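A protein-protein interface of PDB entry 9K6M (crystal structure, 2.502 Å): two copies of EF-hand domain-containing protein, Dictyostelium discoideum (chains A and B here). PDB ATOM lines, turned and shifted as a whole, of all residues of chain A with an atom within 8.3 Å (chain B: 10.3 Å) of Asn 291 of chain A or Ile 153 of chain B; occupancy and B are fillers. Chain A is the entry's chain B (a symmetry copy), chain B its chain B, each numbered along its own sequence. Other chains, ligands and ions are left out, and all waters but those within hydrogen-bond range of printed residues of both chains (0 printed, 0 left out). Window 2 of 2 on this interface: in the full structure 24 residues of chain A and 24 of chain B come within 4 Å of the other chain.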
ATOM      1  N   MET A 284      -3.447  20.066  -7.314  1.00  0.00           N
ATOM      2  CA  MET A 284      -2.535  19.315  -6.472  1.00  0.00           C
ATOM      3  C   MET A 284      -3.343  18.459  -5.492  1.00  0.00           C
ATOM      4  O   MET A 284      -2.977  17.317  -5.211  1.00  0.00           O
ATOM      5  CB  MET A 284      -1.593  20.251  -5.708  1.00  0.00           C
ATOM      6  CG  MET A 284      -0.368  20.670  -6.511  1.00  0.00           C
ATOM      7  SD  MET A 284       0.484  22.107  -5.779  1.00  0.00           S
ATOM      8  CE  MET A 284       1.991  22.214  -6.748  1.00  0.00           C
ATOM      9  N   ASP A 285      -4.487  18.984  -5.028  1.00  0.00           N
ATOM     10  CA  ASP A 285      -5.325  18.258  -4.077  1.00  0.00           C
ATOM     11  C   ASP A 285      -6.052  17.131  -4.793  1.00  0.00           C
ATOM     12  O   ASP A 285      -6.064  16.004  -4.310  1.00  0.00           O
ATOM     13  CB  ASP A 285      -6.257  19.188  -3.304  1.00  0.00           C
ATOM     14  CG  ASP A 285      -5.469  20.176  -2.456  1.00  0.00           C
ATOM     15  OD1 ASP A 285      -4.256  19.915  -2.217  1.00  0.00           O
ATOM     16  OD2 ASP A 285      -6.046  21.229  -2.078  1.00  0.00           O
ATOM     17  N   LEU A 286      -6.596  17.409  -5.972  1.00  0.00           N
ATOM     18  CA  LEU A 286      -7.291  16.374  -6.717  1.00  0.00           C
ATOM     19  C   LEU A 286      -6.338  15.220  -7.036  1.00  0.00           C
ATOM     20  O   LEU A 286      -6.758  14.066  -7.054  1.00  0.00           O
ATOM     21  CB  LEU A 286      -7.875  16.977  -7.997  1.00  0.00           C
ATOM     22  CG  LEU A 286      -9.015  17.987  -7.839  1.00  0.00           C
ATOM     23  CD1 LEU A 286      -9.463  18.484  -9.200  1.00  0.00           C
ATOM     24  CD2 LEU A 286     -10.212  17.373  -7.127  1.00  0.00           C
ATOM     25  N   TYR A 287      -5.049  15.509  -7.256  1.00  0.00           N
ATOM     26  CA  TYR A 287      -4.113  14.447  -7.601  1.00  0.00           C
ATOM     27  C   TYR A 287      -3.752  13.627  -6.362  1.00  0.00           C
ATOM     28  O   TYR A 287      -3.634  12.408  -6.479  1.00  0.00           O
ATOM     29  CB  TYR A 287      -2.883  14.952  -8.359  1.00  0.00           C
ATOM     30  CG  TYR A 287      -3.183  15.079  -9.845  1.00  0.00           C
ATOM     31  CD1 TYR A 287      -3.595  13.969 -10.582  1.00  0.00           C
ATOM     32  CD2 TYR A 287      -3.110  16.300 -10.504  1.00  0.00           C
ATOM     33  CE1 TYR A 287      -3.904  14.058 -11.932  1.00  0.00           C
ATOM     34  CE2 TYR A 287      -3.423  16.408 -11.850  1.00  0.00           C
ATOM     35  CZ  TYR A 287      -3.813  15.288 -12.559  1.00  0.00           C
ATOM     36  OH  TYR A 287      -4.062  15.383 -13.877  1.00  0.00           O
ATOM     37  N   LYS A 288      -3.603  14.277  -5.199  1.00  0.00           N
ATOM     38  CA  LYS A 288      -3.200  13.583  -3.985  1.00  0.00           C
ATOM     39  C   LYS A 288      -4.324  12.621  -3.574  1.00  0.00           C
ATOM     40  O   LYS A 288      -4.093  11.510  -3.074  1.00  0.00           O
ATOM     41  CB  LYS A 288      -2.803  14.607  -2.910  1.00  0.00           C
ATOM     42  CG  LYS A 288      -2.807  14.066  -1.483  1.00  0.00           C
ATOM     43  CD  LYS A 288      -1.749  14.643  -0.546  1.00  0.00           C
ATOM     44  CE  LYS A 288      -1.997  16.070  -0.085  1.00  0.00           C
ATOM     45  NZ  LYS A 288      -0.873  16.581   0.747  1.00  0.00           N
ATOM     46  N   GLY A 289      -5.563  13.031  -3.860  1.00  0.00           N
ATOM     47  CA  GLY A 289      -6.724  12.195  -3.618  1.00  0.00           C
ATOM     48  C   GLY A 289      -6.717  10.894  -4.420  1.00  0.00           C
ATOM     49  O   GLY A 289      -7.474   9.997  -4.082  1.00  0.00           O
ATOM     50  N   ILE A 290      -5.912  10.758  -5.482  1.00  0.00           N
ATOM     51  CA  ILE A 290      -5.807   9.448  -6.110  1.00  0.00           C
ATOM     52  C   ILE A 290      -4.425   8.849  -5.861  1.00  0.00           C
ATOM     53  O   ILE A 290      -4.011   7.928  -6.570  1.00  0.00           O
ATOM     54  CB  ILE A 290      -6.217   9.468  -7.602  1.00  0.00           C
ATOM     55  CG1 ILE A 290      -5.393  10.440  -8.447  1.00  0.00           C
ATOM     56  CG2 ILE A 290      -7.711   9.746  -7.735  1.00  0.00           C
ATOM     57  CD1 ILE A 290      -5.484  10.176  -9.942  1.00  0.00           C
ATOM     58  N   ASN A 291      -3.754   9.299  -4.790  1.00  0.00           N
ATOM     59  CA  ASN A 291      -2.456   8.757  -4.414  1.00  0.00           C
ATOM     60  C   ASN A 291      -1.474   8.997  -5.569  1.00  0.00           C
ATOM     61  O   ASN A 291      -0.597   8.165  -5.870  1.00  0.00           O
ATOM     62  CB  ASN A 291      -2.577   7.288  -3.992  1.00  0.00           C
ATOM     63  CG  ASN A 291      -1.297   6.702  -3.430  1.00  0.00           C
ATOM     64  OD1 ASN A 291      -0.400   7.430  -3.022  1.00  0.00           O
ATOM     65  ND2 ASN A 291      -1.219   5.382  -3.364  1.00  0.00           N
ATOM     66  N   GLN A 292      -1.618  10.174  -6.199  1.00  0.00           N
ATOM     67  CA  GLN A 292      -0.795  10.571  -7.336  1.00  0.00           C
ATOM     68  C   GLN A 292      -0.043  11.856  -6.974  1.00  0.00           C
ATOM     69  O   GLN A 292      -0.651  12.911  -6.823  1.00  0.00           O
ATOM     70  CB  GLN A 292      -1.665  10.722  -8.590  1.00  0.00           C
ATOM     71  CG  GLN A 292      -0.916  11.274  -9.793  1.00  0.00           C
ATOM     72  CD  GLN A 292       0.255  10.422 -10.216  1.00  0.00           C
ATOM     73  OE1 GLN A 292       1.403  10.715  -9.905  1.00  0.00           O
ATOM     74  NE2 GLN A 292      -0.040   9.354 -10.938  1.00  0.00           N
ATOM     75  N   PRO A 293       1.284  11.797  -6.733  1.00  0.00           N
ATOM     76  CA  PRO A 293       2.059  13.000  -6.443  1.00  0.00           C
ATOM     77  C   PRO A 293       2.197  13.902  -7.663  1.00  0.00           C
ATOM     78  O   PRO A 293       2.004  13.455  -8.795  1.00  0.00           O
ATOM     79  CB  PRO A 293       3.435  12.474  -6.014  1.00  0.00           C
ATOM     80  CG  PRO A 293       3.517  11.117  -6.681  1.00  0.00           C
ATOM     81  CD  PRO A 293       2.094  10.580  -6.644  1.00  0.00           C
ATOM     82  N   PHE A 294       2.529  15.175  -7.405  1.00  0.00           N
ATOM     83  CA  PHE A 294       2.504  16.194  -8.443  1.00  0.00           C
ATOM     84  C   PHE A 294       3.853  16.231  -9.159  1.00  0.00           C
ATOM     85  O   PHE A 294       4.710  17.051  -8.814  1.00  0.00           O
ATOM     86  CB  PHE A 294       2.100  17.559  -7.878  1.00  0.00           C
ATOM     87  CG  PHE A 294       1.502  18.456  -8.928  1.00  0.00           C
ATOM     88  CD1 PHE A 294       0.241  18.209  -9.442  1.00  0.00           C
ATOM     89  CD2 PHE A 294       2.225  19.508  -9.457  1.00  0.00           C
ATOM     90  CE1 PHE A 294      -0.304  19.024 -10.421  1.00  0.00           C
ATOM     91  CE2 PHE A 294       1.688  20.312 -10.444  1.00  0.00           C
ATOM     92  CZ  PHE A 294       0.425  20.073 -10.919  1.00  0.00           C
ATOM     93  N   GLU B  58     -12.681   1.051  12.820  1.00  0.00           N
ATOM     94  CA  GLU B  58     -12.680   2.260  12.005  1.00  0.00           C
ATOM     95  C   GLU B  58     -13.671   3.257  12.603  1.00  0.00           C
ATOM     96  O   GLU B  58     -14.599   2.888  13.317  1.00  0.00           O
ATOM     97  CB  GLU B  58     -13.132   1.985  10.571  1.00  0.00           C
ATOM     98  CG  GLU B  58     -12.049   1.457   9.635  1.00  0.00           C
ATOM     99  CD  GLU B  58     -12.508   1.337   8.186  1.00  0.00           C
ATOM    100  OE1 GLU B  58     -11.792   1.826   7.271  1.00  0.00           O
ATOM    101  OE2 GLU B  58     -13.600   0.772   7.972  1.00  0.00           O
ATOM    102  N   SER B 109     -18.163   7.226   6.100  1.00  0.00           N
ATOM    103  CA  SER B 109     -16.818   6.681   6.276  1.00  0.00           C
ATOM    104  C   SER B 109     -15.760   7.755   6.014  1.00  0.00           C
ATOM    105  O   SER B 109     -16.059   8.816   5.462  1.00  0.00           O
ATOM    106  CB  SER B 109     -16.611   5.452   5.370  1.00  0.00           C
ATOM    107  OG  SER B 109     -16.545   5.781   3.984  1.00  0.00           O
ATOM    108  N   PHE B 110     -14.501   7.450   6.359  1.00  0.00           N
ATOM    109  CA  PHE B 110     -13.392   8.387   6.196  1.00  0.00           C
ATOM    110  C   PHE B 110     -13.238   8.759   4.726  1.00  0.00           C
ATOM    111  O   PHE B 110     -13.024   9.925   4.432  1.00  0.00           O
ATOM    112  CB  PHE B 110     -12.079   7.819   6.755  1.00  0.00           C
ATOM    113  CG  PHE B 110     -10.833   8.545   6.303  1.00  0.00           C
ATOM    114  CD1 PHE B 110     -10.459   9.755   6.867  1.00  0.00           C
ATOM    115  CD2 PHE B 110     -10.081   8.058   5.246  1.00  0.00           C
ATOM    116  CE1 PHE B 110      -9.339  10.430   6.413  1.00  0.00           C
ATOM    117  CE2 PHE B 110      -8.968   8.736   4.782  1.00  0.00           C
ATOM    118  CZ  PHE B 110      -8.595   9.920   5.370  1.00  0.00           C
ATOM    119  N   GLY B 111     -13.306   7.763   3.840  1.00  0.00           N
ATOM    120  CA  GLY B 111     -13.215   7.965   2.405  1.00  0.00           C
ATOM    121  C   GLY B 111     -14.377   8.798   1.872  1.00  0.00           C
ATOM    122  O   GLY B 111     -14.150   9.760   1.133  1.00  0.00           O
ATOM    123  N   GLU B 112     -15.599   8.462   2.308  1.00  0.00           N
ATOM    124  CA  GLU B 112     -16.776   9.213   1.922  1.00  0.00           C
ATOM    125  C   GLU B 112     -16.608  10.685   2.299  1.00  0.00           C
ATOM    126  O   GLU B 112     -16.968  11.530   1.487  1.00  0.00           O
ATOM    127  CB  GLU B 112     -18.032   8.600   2.544  1.00  0.00           C
ATOM    128  CG  GLU B 112     -18.507   7.315   1.881  1.00  0.00           C
ATOM    129  CD  GLU B 112     -19.556   6.519   2.673  1.00  0.00           C
ATOM    130  OE1 GLU B 112     -19.790   6.832   3.855  1.00  0.00           O
ATOM    131  OE2 GLU B 112     -20.158   5.554   2.119  1.00  0.00           O
ATOM    132  N   MET B 114     -13.809  12.498   2.959  1.00  0.00           N
ATOM    133  CA  MET B 114     -12.721  13.150   2.250  1.00  0.00           C
ATOM    134  C   MET B 114     -13.185  13.490   0.835  1.00  0.00           C
ATOM    135  O   MET B 114     -12.858  14.558   0.328  1.00  0.00           O
ATOM    136  CB  MET B 114     -11.491  12.238   2.175  1.00  0.00           C
ATOM    137  CG  MET B 114     -10.859  11.903   3.520  1.00  0.00           C
ATOM    138  SD  MET B 114     -10.181  13.311   4.458  1.00  0.00           S
ATOM    139  CE  MET B 114      -9.371  14.221   3.138  1.00  0.00           C
ATOM    140  N   PHE B 115     -13.950  12.581   0.221  1.00  0.00           N
ATOM    141  CA  PHE B 115     -14.482  12.775  -1.117  1.00  0.00           C
ATOM    142  C   PHE B 115     -15.460  13.943  -1.119  1.00  0.00           C
ATOM    143  O   PHE B 115     -15.342  14.826  -1.956  1.00  0.00           O
ATOM    144  CB  PHE B 115     -15.118  11.485  -1.662  1.00  0.00           C
ATOM    145  CG  PHE B 115     -15.586  11.540  -3.099  1.00  0.00           C
ATOM    146  CD1 PHE B 115     -14.763  12.031  -4.107  1.00  0.00           C
ATOM    147  CD2 PHE B 115     -16.842  11.066  -3.448  1.00  0.00           C
ATOM    148  CE1 PHE B 115     -15.193  12.062  -5.427  1.00  0.00           C
ATOM    149  CE2 PHE B 115     -17.274  11.094  -4.765  1.00  0.00           C
ATOM    150  CZ  PHE B 115     -16.449  11.592  -5.755  1.00  0.00           C
ATOM    151  N   VAL B 136     -10.544  11.247 -16.867  1.00  0.00           N
ATOM    152  CA  VAL B 136      -9.256  10.644 -17.143  1.00  0.00           C
ATOM    153  C   VAL B 136      -9.089  10.351 -18.631  1.00  0.00           C
ATOM    154  O   VAL B 136      -7.973  10.487 -19.124  1.00  0.00           O
ATOM    155  CB  VAL B 136      -9.058   9.364 -16.310  1.00  0.00           C
ATOM    156  CG1 VAL B 136      -7.620   8.873 -16.358  1.00  0.00           C
ATOM    157  CG2 VAL B 136      -9.472   9.582 -14.870  1.00  0.00           C
ATOM    158  N   ASN B 145     -17.079   5.211 -13.035  1.00  0.00           N
ATOM    159  CA  ASN B 145     -15.784   4.646 -12.700  1.00  0.00           C
ATOM    160  C   ASN B 145     -14.815   5.770 -12.355  1.00  0.00           C
ATOM    161  O   ASN B 145     -14.084   5.651 -11.384  1.00  0.00           O
ATOM    162  CB  ASN B 145     -15.243   3.739 -13.804  1.00  0.00           C
ATOM    163  CG  ASN B 145     -13.902   3.149 -13.422  1.00  0.00           C
ATOM    164  OD1 ASN B 145     -13.782   2.510 -12.380  1.00  0.00           O
ATOM    165  ND2 ASN B 145     -12.883   3.384 -14.232  1.00  0.00           N
ATOM    166  N   GLU B 146     -14.847   6.862 -13.126  1.00  0.00           N
ATOM    167  CA  GLU B 146     -13.918   7.961 -12.940  1.00  0.00           C
ATOM    168  C   GLU B 146     -14.306   8.727 -11.687  1.00  0.00           C
ATOM    169  O   GLU B 146     -13.433   9.204 -10.974  1.00  0.00           O
ATOM    170  CB  GLU B 146     -13.908   8.889 -14.156  1.00  0.00           C
ATOM    171  CG  GLU B 146     -13.495   8.208 -15.456  1.00  0.00           C
ATOM    172  CD  GLU B 146     -13.721   8.979 -16.752  1.00  0.00           C
ATOM    173  OE1 GLU B 146     -14.863   9.364 -17.042  1.00  0.00           O
ATOM    174  OE2 GLU B 146     -12.767   9.156 -17.498  1.00  0.00           O
ATOM    175  N   PHE B 147     -15.611   8.832 -11.424  1.00  0.00           N
ATOM    176  CA  PHE B 147     -16.093   9.674 -10.340  1.00  0.00           C
ATOM    177  C   PHE B 147     -15.723   9.043  -9.000  1.00  0.00           C
ATOM    178  O   PHE B 147     -15.348   9.780  -8.085  1.00  0.00           O
ATOM    179  CB  PHE B 147     -17.600   9.924 -10.490  1.00  0.00           C
ATOM    180  CG  PHE B 147     -18.189  10.947  -9.548  1.00  0.00           C
ATOM    181  CD1 PHE B 147     -17.906  12.298  -9.695  1.00  0.00           C
ATOM    182  CD2 PHE B 147     -19.032  10.562  -8.514  1.00  0.00           C
ATOM    183  CE1 PHE B 147     -18.421  13.231  -8.813  1.00  0.00           C
ATOM    184  CE2 PHE B 147     -19.566  11.504  -7.648  1.00  0.00           C
ATOM    185  CZ  PHE B 147     -19.250  12.833  -7.793  1.00  0.00           C
ATOM    186  N   ASN B 148     -15.785   7.703  -8.924  1.00  0.00           N
ATOM    187  CA  ASN B 148     -15.555   6.966  -7.687  1.00  0.00           C
ATOM    188  C   ASN B 148     -14.085   6.559  -7.561  1.00  0.00           C
ATOM    189  O   ASN B 148     -13.752   5.684  -6.772  1.00  0.00           O
ATOM    190  CB  ASN B 148     -16.498   5.760  -7.577  1.00  0.00           C
ATOM    191  CG  ASN B 148     -17.965   6.156  -7.506  1.00  0.00           C
ATOM    192  OD1 ASN B 148     -18.772   5.683  -8.298  1.00  0.00           O
ATOM    193  ND2 ASN B 148     -18.328   7.014  -6.561  1.00  0.00           N
ATOM    194  N   SER B 149     -13.210   7.211  -8.332  1.00  0.00           N
ATOM    195  CA  SER B 149     -11.797   6.902  -8.332  1.00  0.00           C
ATOM    196  C   SER B 149     -11.189   7.231  -6.968  1.00  0.00           C
ATOM    197  O   SER B 149     -10.565   6.368  -6.338  1.00  0.00           O
ATOM    198  CB  SER B 149     -11.106   7.631  -9.474  1.00  0.00           C
ATOM    199  OG  SER B 149      -9.699   7.394  -9.491  1.00  0.00           O
ATOM    200  N   ILE B 150     -11.410   8.472  -6.518  1.00  0.00           N
ATOM    201  CA  ILE B 150     -10.864   8.931  -5.256  1.00  0.00           C
ATOM    202  C   ILE B 150     -11.399   8.034  -4.154  1.00  0.00           C
ATOM    203  O   ILE B 150     -10.661   7.645  -3.248  1.00  0.00           O
ATOM    204  CB  ILE B 150     -11.161  10.431  -5.012  1.00  0.00           C
ATOM    205  CG1 ILE B 150     -10.182  11.322  -5.790  1.00  0.00           C
ATOM    206  CG2 ILE B 150     -11.139  10.756  -3.522  1.00  0.00           C
ATOM    207  CD1 ILE B 150     -10.471  12.808  -5.742  1.00  0.00           C
ATOM    208  N   LEU B 151     -12.685   7.698  -4.270  1.00  0.00           N
ATOM    209  CA  LEU B 151     -13.374   6.994  -3.212  1.00  0.00           C
ATOM    210  C   LEU B 151     -12.735   5.625  -3.039  1.00  0.00           C
ATOM    211  O   LEU B 151     -12.342   5.283  -1.945  1.00  0.00           O
ATOM    212  CB  LEU B 151     -14.862   6.905  -3.560  1.00  0.00           C
ATOM    213  CG  LEU B 151     -15.783   6.471  -2.427  1.00  0.00           C
ATOM    214  CD1 LEU B 151     -15.696   7.409  -1.231  1.00  0.00           C
ATOM    215  CD2 LEU B 151     -17.204   6.405  -2.946  1.00  0.00           C
ATOM    216  N   ARG B 152     -12.607   4.865  -4.120  1.00  0.00           N
ATOM    217  CA  ARG B 152     -11.886   3.601  -4.102  1.00  0.00           C
ATOM    218  C   ARG B 152     -10.505   3.752  -3.458  1.00  0.00           C
ATOM    219  O   ARG B 152     -10.148   2.944  -2.613  1.00  0.00           O
ATOM    220  CB  ARG B 152     -11.749   3.044  -5.525  1.00  0.00           C
ATOM    221  CG  ARG B 152     -12.835   2.052  -5.911  1.00  0.00           C
ATOM    222  CD  ARG B 152     -12.649   1.525  -7.321  1.00  0.00           C
ATOM    223  NE  ARG B 152     -13.139   2.453  -8.327  1.00  0.00           N
ATOM    224  CZ  ARG B 152     -12.403   3.092  -9.225  1.00  0.00           C
ATOM    225  NH1 ARG B 152     -11.086   3.064  -9.157  1.00  0.00           N
ATOM    226  NH2 ARG B 152     -12.995   3.829 -10.146  1.00  0.00           N
ATOM    227  N   ILE B 153      -9.720   4.768  -3.846  1.00  0.00           N
ATOM    228  CA  ILE B 153      -8.343   4.866  -3.384  1.00  0.00           C
ATOM    229  C   ILE B 153      -8.303   5.299  -1.913  1.00  0.00           C
ATOM    230  O   ILE B 153      -7.650   4.641  -1.116  1.00  0.00           O
ATOM    231  CB  ILE B 153      -7.523   5.755  -4.346  1.00  0.00           C
ATOM    232  CG1 ILE B 153      -7.492   5.119  -5.738  1.00  0.00           C
ATOM    233  CG2 ILE B 153      -6.119   6.038  -3.833  1.00  0.00           C
ATOM    234  CD1 ILE B 153      -6.905   5.991  -6.814  1.00  0.00           C
ATOM    235  N   LEU B 154      -9.017   6.369  -1.536  1.00  0.00           N
ATOM    236  CA  LEU B 154      -9.027   6.837  -0.154  1.00  0.00           C
ATOM    237  C   LEU B 154      -9.698   5.818   0.767  1.00  0.00           C
ATOM    238  O   LEU B 154      -9.543   5.898   1.983  1.00  0.00           O
ATOM    239  CB  LEU B 154      -9.745   8.189  -0.064  1.00  0.00           C
ATOM    240  CG  LEU B 154      -9.076   9.330  -0.831  1.00  0.00           C
ATOM    241  CD1 LEU B 154      -9.704  10.673  -0.488  1.00  0.00           C
ATOM    242  CD2 LEU B 154      -7.564   9.366  -0.573  1.00  0.00           C
ATOM    243  N   SER B 155     -10.463   4.879   0.201  1.00  0.00           N
ATOM    244  CA  SER B 155     -11.181   3.906   1.006  1.00  0.00           C
ATOM    245  C   SER B 155     -10.367   2.624   1.093  1.00  0.00           C
ATOM    246  O   SER B 155     -10.195   2.085   2.177  1.00  0.00           O
ATOM    247  CB  SER B 155     -12.570   3.614   0.478  1.00  0.00           C
ATOM    248  OG  SER B 155     -13.462   4.717   0.650  1.00  0.00           O
ATOM    249  N   ASN B 156      -9.880   2.132  -0.053  1.00  0.00           N
ATOM    250  CA  ASN B 156      -9.049   0.936  -0.093  1.00  0.00           C
ATOM    251  C   ASN B 156      -7.636   1.287   0.377  1.00  0.00           C
ATOM    252  O   ASN B 156      -6.666   1.071  -0.347  1.00  0.00           O
ATOM    253  CB  ASN B 156      -9.019   0.279  -1.481  1.00  0.00           C
ATOM    254  CG  ASN B 156     -10.368  -0.240  -1.938  1.00  0.00           C
ATOM    255  OD1 ASN B 156     -11.373  -0.094  -1.241  1.00  0.00           O
ATOM    256  ND2 ASN B 156     -10.405  -0.842  -3.117  1.00  0.00           N
ATOM    257  N   GLN B 157      -7.538   1.813   1.606  1.00  0.00           N
ATOM    258  CA  GLN B 157      -6.270   2.194   2.212  1.00  0.00           C
ATOM    259  C   GLN B 157      -5.505   3.133   1.268  1.00  0.00           C
ATOM    260  O   GLN B 157      -5.499   4.348   1.549  1.00  0.00           O
ATOM    261  CB  GLN B 157      -5.446   0.950   2.560  1.00  0.00           C
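Among the printed residues, pairs that only touch across the chains: Gly 289 of chain A with Ile 150 of chain B (3.5 Å), Gly 289 of chain A with Leu 154 of chain B (3.6 Å), Ile 290 of chain A with Ser 149 of chain B (3.5 Å), Ile 290 of chain A with Ile 150 of chain B (3.5 Å), Ile 290 of chain A with Ile 153 of chain B (3.5 Å) and Asn 291 of chain A with Ile 153 of chain B (3.8 Å).
Gly 289 of chain A touches just these residues of chain B: Ile 150 and Leu 154.
Of chain B, only Ser 149 (3.5 Å), Ile 150 (3.5 Å) and Ile 153 (3.5 Å) come within 4 Å of Ile 290 of chain A.
Asn 291 of chain A touches just one residue of chain B: Ile 153 (3.8 Å).
No residue of chain B comes within 4 Å of Gln 292 of chain A.
Ser 109 of chain B touches none of the printed residues of chain A.
Of the printed residues of chain A, Ser 149 of chain B touches Ile 290 (3.5 Å).
Of the printed residues of chain A, Ile 150 of chain B touches Gly 289 (3.5 Å) and Ile 290 (3.5 Å).
Ile 153 of chain B touches two residues of chain A.
Of the printed residues of chain A, Leu 154 of chain B touches Gly 289 (3.6 Å).
Among the printed residues, no Asp or Glu carboxylate lies within 4 Å of a Lys or Arg side-chain nitrogen of the other chain.
No position is printed for both chains.
Of the 6 pairs that touch across the chains among the printed residues, none has its exchanged pair printed and touching as well.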
